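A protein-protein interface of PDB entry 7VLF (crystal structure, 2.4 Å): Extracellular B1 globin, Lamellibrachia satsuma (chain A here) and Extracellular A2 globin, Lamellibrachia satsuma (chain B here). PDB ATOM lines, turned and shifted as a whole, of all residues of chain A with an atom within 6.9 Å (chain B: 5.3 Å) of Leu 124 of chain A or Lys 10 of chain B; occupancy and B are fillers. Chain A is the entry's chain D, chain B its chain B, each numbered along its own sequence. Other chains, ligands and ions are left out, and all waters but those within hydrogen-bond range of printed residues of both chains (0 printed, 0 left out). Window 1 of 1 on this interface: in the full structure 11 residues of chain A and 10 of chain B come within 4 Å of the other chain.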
ATOM      1  N   GLN A  15      -6.597  23.137   1.526  1.00  0.00           N
ATOM      2  CA  GLN A  15      -5.189  22.837   1.285  1.00  0.00           C
ATOM      3  C   GLN A  15      -4.971  22.226  -0.093  1.00  0.00           C
ATOM      4  O   GLN A  15      -3.884  22.364  -0.665  1.00  0.00           O
ATOM      5  CB  GLN A  15      -4.654  21.911   2.377  1.00  0.00           C
ATOM      6  CG  GLN A  15      -4.665  22.542   3.766  1.00  0.00           C
ATOM      7  CD  GLN A  15      -4.085  21.634   4.832  1.00  0.00           C
ATOM      8  OE1 GLN A  15      -3.783  22.075   5.942  1.00  0.00           O
ATOM      9  NE2 GLN A  15      -3.931  20.358   4.504  1.00  0.00           N
ATOM     10  N   GLN A  18      -4.956  25.113  -2.638  1.00  0.00           N
ATOM     11  CA  GLN A  18      -3.740  25.917  -2.545  1.00  0.00           C
ATOM     12  C   GLN A  18      -2.712  25.491  -3.584  1.00  0.00           C
ATOM     13  O   GLN A  18      -2.014  26.332  -4.160  1.00  0.00           O
ATOM     14  CB  GLN A  18      -3.154  25.808  -1.137  1.00  0.00           C
ATOM     15  CG  GLN A  18      -1.811  26.494  -0.961  1.00  0.00           C
ATOM     16  CD  GLN A  18      -1.178  26.188   0.381  1.00  0.00           C
ATOM     17  OE1 GLN A  18      -0.183  26.801   0.768  1.00  0.00           O
ATOM     18  NE2 GLN A  18      -1.755  25.234   1.099  1.00  0.00           N
ATOM     19  N   ILE A  19      -2.609  24.189  -3.842  1.00  0.00           N
ATOM     20  CA  ILE A  19      -1.614  23.659  -4.768  1.00  0.00           C
ATOM     21  C   ILE A  19      -2.207  23.212  -6.093  1.00  0.00           C
ATOM     22  O   ILE A  19      -1.441  22.842  -6.996  1.00  0.00           O
ATOM     23  CB  ILE A  19      -0.821  22.497  -4.137  1.00  0.00           C
ATOM     24  CG1 ILE A  19      -1.778  21.381  -3.714  1.00  0.00           C
ATOM     25  CG2 ILE A  19      -0.002  22.988  -2.961  1.00  0.00           C
ATOM     26  CD1 ILE A  19      -1.280  19.990  -4.051  1.00  0.00           C
ATOM     27  N   THR A  31       5.299  18.490 -13.251  1.00  0.00           N
ATOM     28  CA  THR A  31       6.133  18.124 -12.114  1.00  0.00           C
ATOM     29  C   THR A  31       5.367  17.242 -11.136  1.00  0.00           C
ATOM     30  O   THR A  31       5.930  16.308 -10.554  1.00  0.00           O
ATOM     31  CB  THR A  31       6.641  19.393 -11.417  1.00  0.00           C
ATOM     32  OG1 THR A  31       7.405  20.178 -12.342  1.00  0.00           O
ATOM     33  CG2 THR A  31       7.507  19.065 -10.214  1.00  0.00           C
ATOM     34  N   MET A  32       4.079  17.531 -10.935  1.00  0.00           N
ATOM     35  CA  MET A  32       3.266  16.715 -10.038  1.00  0.00           C
ATOM     36  C   MET A  32       2.993  15.334 -10.629  1.00  0.00           C
ATOM     37  O   MET A  32       3.042  14.326  -9.914  1.00  0.00           O
ATOM     38  CB  MET A  32       1.953  17.435  -9.728  1.00  0.00           C
ATOM     39  CG  MET A  32       2.129  18.775  -9.027  1.00  0.00           C
ATOM     40  SD  MET A  32       0.566  19.655  -8.825  1.00  0.00           S
ATOM     41  CE  MET A  32      -0.364  18.476  -7.846  1.00  0.00           C
ATOM     42  N   ILE A  36       4.681  11.926  -8.779  1.00  0.00           N
ATOM     43  CA  ILE A  36       3.751  11.018  -8.122  1.00  0.00           C
ATOM     44  C   ILE A  36       3.792   9.642  -8.777  1.00  0.00           C
ATOM     45  O   ILE A  36       3.763   8.609  -8.095  1.00  0.00           O
ATOM     46  CB  ILE A  36       2.335  11.610  -8.152  1.00  0.00           C
ATOM     47  CG1 ILE A  36       2.278  12.845  -7.247  1.00  0.00           C
ATOM     48  CG2 ILE A  36       1.313  10.578  -7.730  1.00  0.00           C
ATOM     49  CD1 ILE A  36       0.916  13.504  -7.197  1.00  0.00           C
ATOM     50  N   THR A 119       2.839  11.083   1.117  1.00  0.00           N
ATOM     51  CA  THR A 119       4.239  11.470   1.195  1.00  0.00           C
ATOM     52  C   THR A 119       4.612  12.580   0.226  1.00  0.00           C
ATOM     53  O   THR A 119       5.478  13.396   0.545  1.00  0.00           O
ATOM     54  CB  THR A 119       5.139  10.254   0.938  1.00  0.00           C
ATOM     55  OG1 THR A 119       4.665   9.144   1.710  1.00  0.00           O
ATOM     56  CG2 THR A 119       6.573  10.554   1.339  1.00  0.00           C
ATOM     57  N   VAL A 120       3.963  12.645  -0.938  1.00  0.00           N
ATOM     58  CA  VAL A 120       4.288  13.680  -1.914  1.00  0.00           C
ATOM     59  C   VAL A 120       3.752  15.032  -1.462  1.00  0.00           C
ATOM     60  O   VAL A 120       4.456  16.048  -1.516  1.00  0.00           O
ATOM     61  CB  VAL A 120       3.747  13.292  -3.303  1.00  0.00           C
ATOM     62  CG1 VAL A 120       3.714  14.504  -4.218  1.00  0.00           C
ATOM     63  CG2 VAL A 120       4.600  12.191  -3.913  1.00  0.00           C
ATOM     64  N   LEU A 121       2.503  15.063  -0.999  1.00  0.00           N
ATOM     65  CA  LEU A 121       1.863  16.332  -0.662  1.00  0.00           C
ATOM     66  C   LEU A 121       2.540  17.109   0.467  1.00  0.00           C
ATOM     67  O   LEU A 121       2.579  18.349   0.373  1.00  0.00           O
ATOM     68  CB  LEU A 121       0.385  16.089  -0.331  1.00  0.00           C
ATOM     69  CG  LEU A 121      -0.480  15.529  -1.460  1.00  0.00           C
ATOM     70  CD1 LEU A 121      -1.955  15.622  -1.099  1.00  0.00           C
ATOM     71  CD2 LEU A 121      -0.196  16.245  -2.773  1.00  0.00           C
ATOM     72  N   PRO A 122       3.057  16.491   1.540  1.00  0.00           N
ATOM     73  CA  PRO A 122       3.688  17.294   2.605  1.00  0.00           C
ATOM     74  C   PRO A 122       4.779  18.245   2.129  1.00  0.00           C
ATOM     75  O   PRO A 122       5.001  19.280   2.773  1.00  0.00           O
ATOM     76  CB  PRO A 122       4.253  16.225   3.548  1.00  0.00           C
ATOM     77  CG  PRO A 122       3.320  15.093   3.402  1.00  0.00           C
ATOM     78  CD  PRO A 122       2.918  15.080   1.953  1.00  0.00           C
ATOM     79  N   SER A 123       5.463  17.941   1.027  1.00  0.00           N
ATOM     80  CA  SER A 123       6.511  18.808   0.503  1.00  0.00           C
ATOM     81  C   SER A 123       5.976  19.895  -0.422  1.00  0.00           C
ATOM     82  O   SER A 123       6.773  20.602  -1.048  1.00  0.00           O
ATOM     83  CB  SER A 123       7.567  17.979  -0.236  1.00  0.00           C
ATOM     84  OG  SER A 123       8.290  17.148   0.659  1.00  0.00           O
ATOM     85  N   LEU A 124       4.655  20.045  -0.522  1.00  0.00           N
ATOM     86  CA  LEU A 124       4.067  21.049  -1.401  1.00  0.00           C
ATOM     87  C   LEU A 124       3.064  21.931  -0.669  1.00  0.00           C
ATOM     88  O   LEU A 124       2.929  23.114  -0.991  1.00  0.00           O
ATOM     89  CB  LEU A 124       3.384  20.371  -2.599  1.00  0.00           C
ATOM     90  CG  LEU A 124       4.286  19.597  -3.561  1.00  0.00           C
ATOM     91  CD1 LEU A 124       3.464  19.002  -4.693  1.00  0.00           C
ATOM     92  CD2 LEU A 124       5.384  20.495  -4.104  1.00  0.00           C
ATOM     93  N   ILE A 125       2.364  21.373   0.317  1.00  0.00           N
ATOM     94  CA  ILE A 125       1.310  22.081   1.037  1.00  0.00           C
ATOM     95  C   ILE A 125       1.851  22.563   2.375  1.00  0.00           C
ATOM     96  O   ILE A 125       2.588  21.842   3.060  1.00  0.00           O
ATOM     97  CB  ILE A 125       0.075  21.180   1.231  1.00  0.00           C
ATOM     98  CG1 ILE A 125      -0.444  20.691  -0.123  1.00  0.00           C
ATOM     99  CG2 ILE A 125      -1.024  21.920   1.983  1.00  0.00           C
ATOM    100  CD1 ILE A 125      -1.718  19.876  -0.034  1.00  0.00           C
ATOM    101  N   ASP A 126       1.485  23.788   2.748  1.00  0.00           N
ATOM    102  CA  ASP A 126       1.871  24.348   4.035  1.00  0.00           C
ATOM    103  C   ASP A 126       1.006  23.758   5.139  1.00  0.00           C
ATOM    104  O   ASP A 126      -0.226  23.771   5.047  1.00  0.00           O
ATOM    105  CB  ASP A 126       1.731  25.869   4.016  1.00  0.00           C
ATOM    106  CG  ASP A 126       2.503  26.508   2.888  1.00  0.00           C
ATOM    107  OD1 ASP A 126       3.203  25.775   2.159  1.00  0.00           O
ATOM    108  OD2 ASP A 126       2.406  27.743   2.721  1.00  0.00           O
ATOM    109  N   ASN A 127       1.656  23.253   6.185  1.00  0.00           N
ATOM    110  CA  ASN A 127       0.984  22.657   7.339  1.00  0.00           C
ATOM    111  C   ASN A 127       0.002  21.571   6.902  1.00  0.00           C
ATOM    112  O   ASN A 127      -1.201  21.624   7.170  1.00  0.00           O
ATOM    113  CB  ASN A 127       0.287  23.729   8.180  1.00  0.00           C
ATOM    114  CG  ASN A 127       0.969  23.951   9.514  1.00  0.00           C
ATOM    115  OD1 ASN A 127       1.335  22.999  10.204  1.00  0.00           O
ATOM    116  ND2 ASN A 127       1.155  25.213   9.880  1.00  0.00           N
ATOM    117  N   PHE A 128       0.548  20.575   6.207  1.00  0.00           N
ATOM    118  CA  PHE A 128      -0.242  19.430   5.776  1.00  0.00           C
ATOM    119  C   PHE A 128      -0.823  18.703   6.983  1.00  0.00           C
ATOM    120  O   PHE A 128      -0.136  18.471   7.981  1.00  0.00           O
ATOM    121  CB  PHE A 128       0.631  18.489   4.943  1.00  0.00           C
ATOM    122  CG  PHE A 128      -0.041  17.200   4.564  1.00  0.00           C
ATOM    123  CD1 PHE A 128      -0.957  17.157   3.528  1.00  0.00           C
ATOM    124  CD2 PHE A 128       0.265  16.025   5.229  1.00  0.00           C
ATOM    125  CE1 PHE A 128      -1.567  15.968   3.173  1.00  0.00           C
ATOM    126  CE2 PHE A 128      -0.341  14.834   4.878  1.00  0.00           C
ATOM    127  CZ  PHE A 128      -1.258  14.805   3.849  1.00  0.00           C
ATOM    128  N   LEU B   6       9.847  19.241  -6.340  1.00  0.00           N
ATOM    129  CA  LEU B   6       8.812  19.569  -5.364  1.00  0.00           C
ATOM    130  C   LEU B   6       9.265  20.690  -4.440  1.00  0.00           C
ATOM    131  O   LEU B   6       8.496  21.614  -4.151  1.00  0.00           O
ATOM    132  CB  LEU B   6       8.445  18.327  -4.555  1.00  0.00           C
ATOM    133  CG  LEU B   6       8.010  17.094  -5.342  1.00  0.00           C
ATOM    134  CD1 LEU B   6       7.687  15.956  -4.389  1.00  0.00           C
ATOM    135  CD2 LEU B   6       6.814  17.414  -6.228  1.00  0.00           C
ATOM    136  N   GLN B   7      10.508  20.623  -3.965  1.00  0.00           N
ATOM    137  CA  GLN B   7      11.037  21.681  -3.114  1.00  0.00           C
ATOM    138  C   GLN B   7      11.079  23.012  -3.853  1.00  0.00           C
ATOM    139  O   GLN B   7      10.992  24.073  -3.227  1.00  0.00           O
ATOM    140  CB  GLN B   7      12.430  21.299  -2.609  1.00  0.00           C
ATOM    141  CG  GLN B   7      12.481  20.059  -1.711  1.00  0.00           C
ATOM    142  CD  GLN B   7      12.198  18.761  -2.450  1.00  0.00           C
ATOM    143  OE1 GLN B   7      12.159  18.731  -3.680  1.00  0.00           O
ATOM    144  NE2 GLN B   7      11.986  17.687  -1.702  1.00  0.00           N
ATOM    145  N   ARG B   8      11.216  22.973  -5.179  1.00  0.00           N
ATOM    146  CA  ARG B   8      11.111  24.191  -5.973  1.00  0.00           C
ATOM    147  C   ARG B   8       9.704  24.769  -5.897  1.00  0.00           C
ATOM    148  O   ARG B   8       9.524  25.961  -5.622  1.00  0.00           O
ATOM    149  CB  ARG B   8      11.496  23.904  -7.425  1.00  0.00           C
ATOM    150  CG  ARG B   8      12.989  23.931  -7.692  1.00  0.00           C
ATOM    151  CD  ARG B   8      13.338  23.133  -8.937  1.00  0.00           C
ATOM    152  NE  ARG B   8      14.594  23.570  -9.540  1.00  0.00           N
ATOM    153  CZ  ARG B   8      15.798  23.244  -9.086  1.00  0.00           C
ATOM    154  NH1 ARG B   8      15.918  22.477  -8.011  1.00  0.00           N
ATOM    155  NH2 ARG B   8      16.884  23.687  -9.702  1.00  0.00           N
ATOM    156  N   LEU B   9       8.692  23.929  -6.124  1.00  0.00           N
ATOM    157  CA  LEU B   9       7.313  24.407  -6.174  1.00  0.00           C
ATOM    158  C   LEU B   9       6.908  25.076  -4.866  1.00  0.00           C
ATOM    159  O   LEU B   9       6.286  26.145  -4.869  1.00  0.00           O
ATOM    160  CB  LEU B   9       6.371  23.246  -6.499  1.00  0.00           C
ATOM    161  CG  LEU B   9       6.547  22.566  -7.857  1.00  0.00           C
ATOM    162  CD1 LEU B   9       5.562  21.418  -8.005  1.00  0.00           C
ATOM    163  CD2 LEU B   9       6.373  23.570  -8.984  1.00  0.00           C
ATOM    164  N   LYS B  10       7.255  24.461  -3.734  1.00  0.00           N
ATOM    165  CA  LYS B  10       6.884  25.025  -2.440  1.00  0.00           C
ATOM    166  C   LYS B  10       7.616  26.335  -2.178  1.00  0.00           C
ATOM    167  O   LYS B  10       7.055  27.255  -1.571  1.00  0.00           O
ATOM    168  CB  LYS B  10       7.168  24.016  -1.329  1.00  0.00           C
ATOM    169  CG  LYS B  10       6.565  24.384   0.017  1.00  0.00           C
ATOM    170  CD  LYS B  10       6.640  23.218   0.990  1.00  0.00           C
ATOM    171  CE  LYS B  10       5.891  23.523   2.276  1.00  0.00           C
ATOM    172  NZ  LYS B  10       5.843  22.340   3.181  1.00  0.00           N
ATOM    173  N   VAL B  11       8.863  26.444  -2.639  1.00  0.00           N
ATOM    174  CA  VAL B  11       9.612  27.684  -2.464  1.00  0.00           C
ATOM    175  C   VAL B  11       8.983  28.812  -3.279  1.00  0.00           C
ATOM    176  O   VAL B  11       8.892  29.955  -2.814  1.00  0.00           O
ATOM    177  CB  VAL B  11      11.093  27.465  -2.833  1.00  0.00           C
ATOM    178  CG1 VAL B  11      11.784  28.784  -3.137  1.00  0.00           C
ATOM    179  CG2 VAL B  11      11.821  26.746  -1.701  1.00  0.00           C
ATOM    180  N   LYS B  12       8.527  28.512  -4.498  1.00  0.00           N
ATOM    181  CA  LYS B  12       7.941  29.545  -5.349  1.00  0.00           C
ATOM    182  C   LYS B  12       6.719  30.177  -4.693  1.00  0.00           C
ATOM    183  O   LYS B  12       6.620  31.404  -4.577  1.00  0.00           O
ATOM    184  CB  LYS B  12       7.561  28.946  -6.702  1.00  0.00           C
ATOM    185  CG  LYS B  12       8.731  28.363  -7.464  1.00  0.00           C
ATOM    186  CD  LYS B  12       8.272  27.588  -8.684  1.00  0.00           C
ATOM    187  CE  LYS B  12       8.962  28.111  -9.927  1.00  0.00           C
ATOM    188  NZ  LYS B  12       8.028  28.772 -10.881  1.00  0.00           N
ATOM    189  N   ARG B  13       5.763  29.344  -4.274  1.00  0.00           N
ATOM    190  CA  ARG B  13       4.534  29.858  -3.682  1.00  0.00           C
ATOM    191  C   ARG B  13       4.817  30.618  -2.394  1.00  0.00           C
ATOM    192  O   ARG B  13       4.170  31.632  -2.109  1.00  0.00           O
ATOM    193  CB  ARG B  13       3.564  28.707  -3.426  1.00  0.00           C
ATOM    194  CG  ARG B  13       2.262  29.124  -2.761  1.00  0.00           C
ATOM    195  CD  ARG B  13       1.331  27.936  -2.592  1.00  0.00           C
ATOM    196  NE  ARG B  13       2.036  26.763  -2.090  1.00  0.00           N
ATOM    197  CZ  ARG B  13       2.387  26.594  -0.821  1.00  0.00           C
ATOM    198  NH1 ARG B  13       3.021  25.491  -0.452  1.00  0.00           N
ATOM    199  NH2 ARG B  13       2.109  27.532   0.074  1.00  0.00           N
ATOM    200  N   GLN B  14       5.783  30.147  -1.603  1.00  0.00           N
ATOM    201  CA  GLN B  14       6.114  30.837  -0.360  1.00  0.00           C
ATOM    202  C   GLN B  14       6.821  32.161  -0.620  1.00  0.00           C
ATOM    203  O   GLN B  14       6.631  33.120   0.138  1.00  0.00           O
ATOM    204  CB  GLN B  14       6.972  29.938   0.531  1.00  0.00           C
ATOM    205  CG  GLN B  14       6.211  28.781   1.164  1.00  0.00           C
ATOM    206  CD  GLN B  14       7.019  28.066   2.230  1.00  0.00           C
ATOM    207  OE1 GLN B  14       8.235  28.234   2.319  1.00  0.00           O
ATOM    208  NE2 GLN B  14       6.345  27.267   3.048  1.00  0.00           N
ATOM    209  N   TRP B  15       7.632  32.242  -1.677  1.00  0.00           N
ATOM    210  CA  TRP B  15       8.285  33.506  -2.000  1.00  0.00           C
ATOM    211  C   TRP B  15       7.273  34.535  -2.485  1.00  0.00           C
ATOM    212  O   TRP B  15       7.294  35.691  -2.046  1.00  0.00           O
ATOM    213  CB  TRP B  15       9.377  33.288  -3.047  1.00  0.00           C
ATOM    214  CG  TRP B  15       9.849  34.561  -3.681  1.00  0.00           C
ATOM    215  CD1 TRP B  15       9.480  35.052  -4.897  1.00  0.00           C
ATOM    216  CD2 TRP B  15      10.768  35.512  -3.129  1.00  0.00           C
ATOM    217  NE1 TRP B  15      10.112  36.246  -5.141  1.00  0.00           N
ATOM    218  CE2 TRP B  15      10.911  36.551  -4.071  1.00  0.00           C
ATOM    219  CE3 TRP B  15      11.488  35.584  -1.932  1.00  0.00           C
ATOM    220  CZ2 TRP B  15      11.741  37.647  -3.853  1.00  0.00           C
ATOM    221  CZ3 TRP B  15      12.311  36.674  -1.719  1.00  0.00           C
ATOM    222  CH2 TRP B  15      12.431  37.691  -2.674  1.00  0.00           C
ATOM    223  N   VAL B 124       4.635  27.242   8.714  1.00  0.00           N
ATOM    224  CA  VAL B 124       4.568  26.832   7.315  1.00  0.00           C
ATOM    225  C   VAL B 124       5.923  26.855   6.628  1.00  0.00           C
ATOM    226  O   VAL B 124       6.031  26.368   5.489  1.00  0.00           O
ATOM    227  CB  VAL B 124       3.564  27.698   6.524  1.00  0.00           C
ATOM    228  CG1 VAL B 124       2.184  27.616   7.156  1.00  0.00           C
ATOM    229  CG2 VAL B 124       4.043  29.141   6.461  1.00  0.00           C
ATOM    230  N   ASP B 126       9.696  25.994   5.421  1.00  0.00           N
ATOM    231  CA  ASP B 126      10.402  24.753   5.107  1.00  0.00           C
ATOM    232  C   ASP B 126      11.884  25.082   4.956  1.00  0.00           C
ATOM    233  O   ASP B 126      12.328  25.496   3.881  1.00  0.00           O
ATOM    234  CB  ASP B 126       9.839  24.114   3.840  1.00  0.00           C
ATOM    235  CG  ASP B 126      10.286  22.673   3.657  1.00  0.00           C
ATOM    236  OD1 ASP B 126      11.444  22.349   3.996  1.00  0.00           O
ATOM    237  OD2 ASP B 126       9.469  21.861   3.172  1.00  0.00           O
ATOM    238  N   TRP B 130      14.228  25.295   1.532  1.00  0.00           N
ATOM    239  CA  TRP B 130      14.757  26.627   1.260  1.00  0.00           C
ATOM    240  C   TRP B 130      16.281  26.647   1.262  1.00  0.00           C
ATOM    241  O   TRP B 130      16.893  27.272   0.389  1.00  0.00           O
ATOM    242  CB  TRP B 130      14.209  27.629   2.275  1.00  0.00           C
ATOM    243  CG  TRP B 130      12.907  28.238   1.853  1.00  0.00           C
ATOM    244  CD1 TRP B 130      11.654  27.765   2.118  1.00  0.00           C
ATOM    245  CD2 TRP B 130      12.729  29.429   1.077  1.00  0.00           C
ATOM    246  NE1 TRP B 130      10.708  28.591   1.561  1.00  0.00           N
ATOM    247  CE2 TRP B 130      11.343  29.620   0.916  1.00  0.00           C
ATOM    248  CE3 TRP B 130      13.608  30.355   0.506  1.00  0.00           C
ATOM    249  CZ2 TRP B 130      10.814  30.697   0.208  1.00  0.00           C
ATOM    250  CZ3 TRP B 130      13.081  31.424  -0.197  1.00  0.00           C
ATOM    251  CH2 TRP B 130      11.697  31.587  -0.339  1.00  0.00           C
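The side-chain amino group of Lys 10 of chain B is in hydrogen-bond range of the backbone carbonyl oxygen of Pro 122 of chain A (3.2 Å). The side-chain amino group (NZ) of Lys 10 of chain B sits at hydrogen-bond distance from the backbone carbonyl oxygen (O) of Ile 125 of chain A, 3.3 Å away. OE1 of Gln 18 of chain A lies within hydrogen-bond range of NH2 of Arg 13 of chain B (2.5 Å). The backbone carbonyl oxygen (O) of Leu 124 of chain A lies within hydrogen-bond range of the guanidinium group (NH1) of Arg 13 of chain B (2.4 Å). OD1 of Asp 126 of chain A is in salt-bridge range of NH1 of Arg 13 of chain B (2.6 Å).
The side-chain amino group (NZ) of Lys 10 of chain B is in salt-bridge range of the side-chain carboxylate (OD2) of Asp 126 of chain B. NE2 of Gln 14 of chain B lies within hydrogen-bond range of O of Val 124 of chain B, at 2.6 Å. The side-chain amide oxygen of Gln 14 of chain B sits at hydrogen-bond distance from the indole nitrogen of Trp 130 of chain B (2.6 Å). The side-chain amide oxygen (OE1) of Gln 15 of chain A lies close to the backbone carbonyl oxygen (O) of Asn 127 of chain A (2.9 Å). OE1 of Gln 18 of chain A lies close to OD2 of Asp 126 of chain A, 3.4 Å away.
Leu 9 of chain B touches Thr 31 of chain A (CD1 to CG2, 3.8 Å). Leu 6 of chain B touches Ser 123 of chain A (O to O, 3.7 Å). CD of Lys 10 of chain B touches O of Ser 123 of chain A, at 3.3 Å. Leu 124 of chain A touches Leu 6 of chain B. Leu 124 of chain A touches Leu 9 of chain B. O of Leu 124 of chain A touches CG of Lys 10 of chain B, 3.98 Å away. Asp 126 of chain A touches Lys 10 of chain B (OD1 to CE, 3.5 Å). OD1 of Asp 126 of chain A touches NE2 of Gln 14 of chain B, at 3.6 Å. Val 124 of chain B touches Asp 126 of chain A. Asn 127 of chain A touches Val 124 of chain B (ND2 to CG1, 3.8 Å).
Printed residues of chain B within 4 Å of Leu 124 of chain A: Leu 6 (3.3 Å), Leu 9 (3.8 Å), Lys 10 (3.98 Å) and Arg 13 (2.4 Å). Of the printed residues of chain A, Lys 10 of chain B touches Pro 122, Ser 123, Leu 124, Ile 125 and Asp 126. Printed residues of chain A within 4 Å of Leu 9 of chain B: Thr 31 (3.8 Å) and Leu 124 (3.8 Å). Of the printed residues of chain A, Arg 13 of chain B touches Gln 18 (2.5 Å), Leu 124 (2.4 Å) and Asp 126 (2.6 Å). The nearest printed residue of chain B that does not touch Leu 124 of chain A is Gln 7 of chain B (5.1 Å). The nearest printed residue of chain B that does not touch Ser 123 of chain A is Gln 7 of chain B (4.4 Å).
Of the 16 printed residues of chain A, 8 touch a printed residue of chain B. Hydrophobic or aromatic side chains of chain B within 4 Å of the printed part of chain A: Leu 6, Leu 9 and Val 124. Among the printed residues, 15 pairs touch across the chains. Among the printed residues, Asp or Glu carboxylates within 4 Å of a Lys or Arg side-chain nitrogen of the other chain: Asp 126 of chain A with Arg 13 of chain B.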
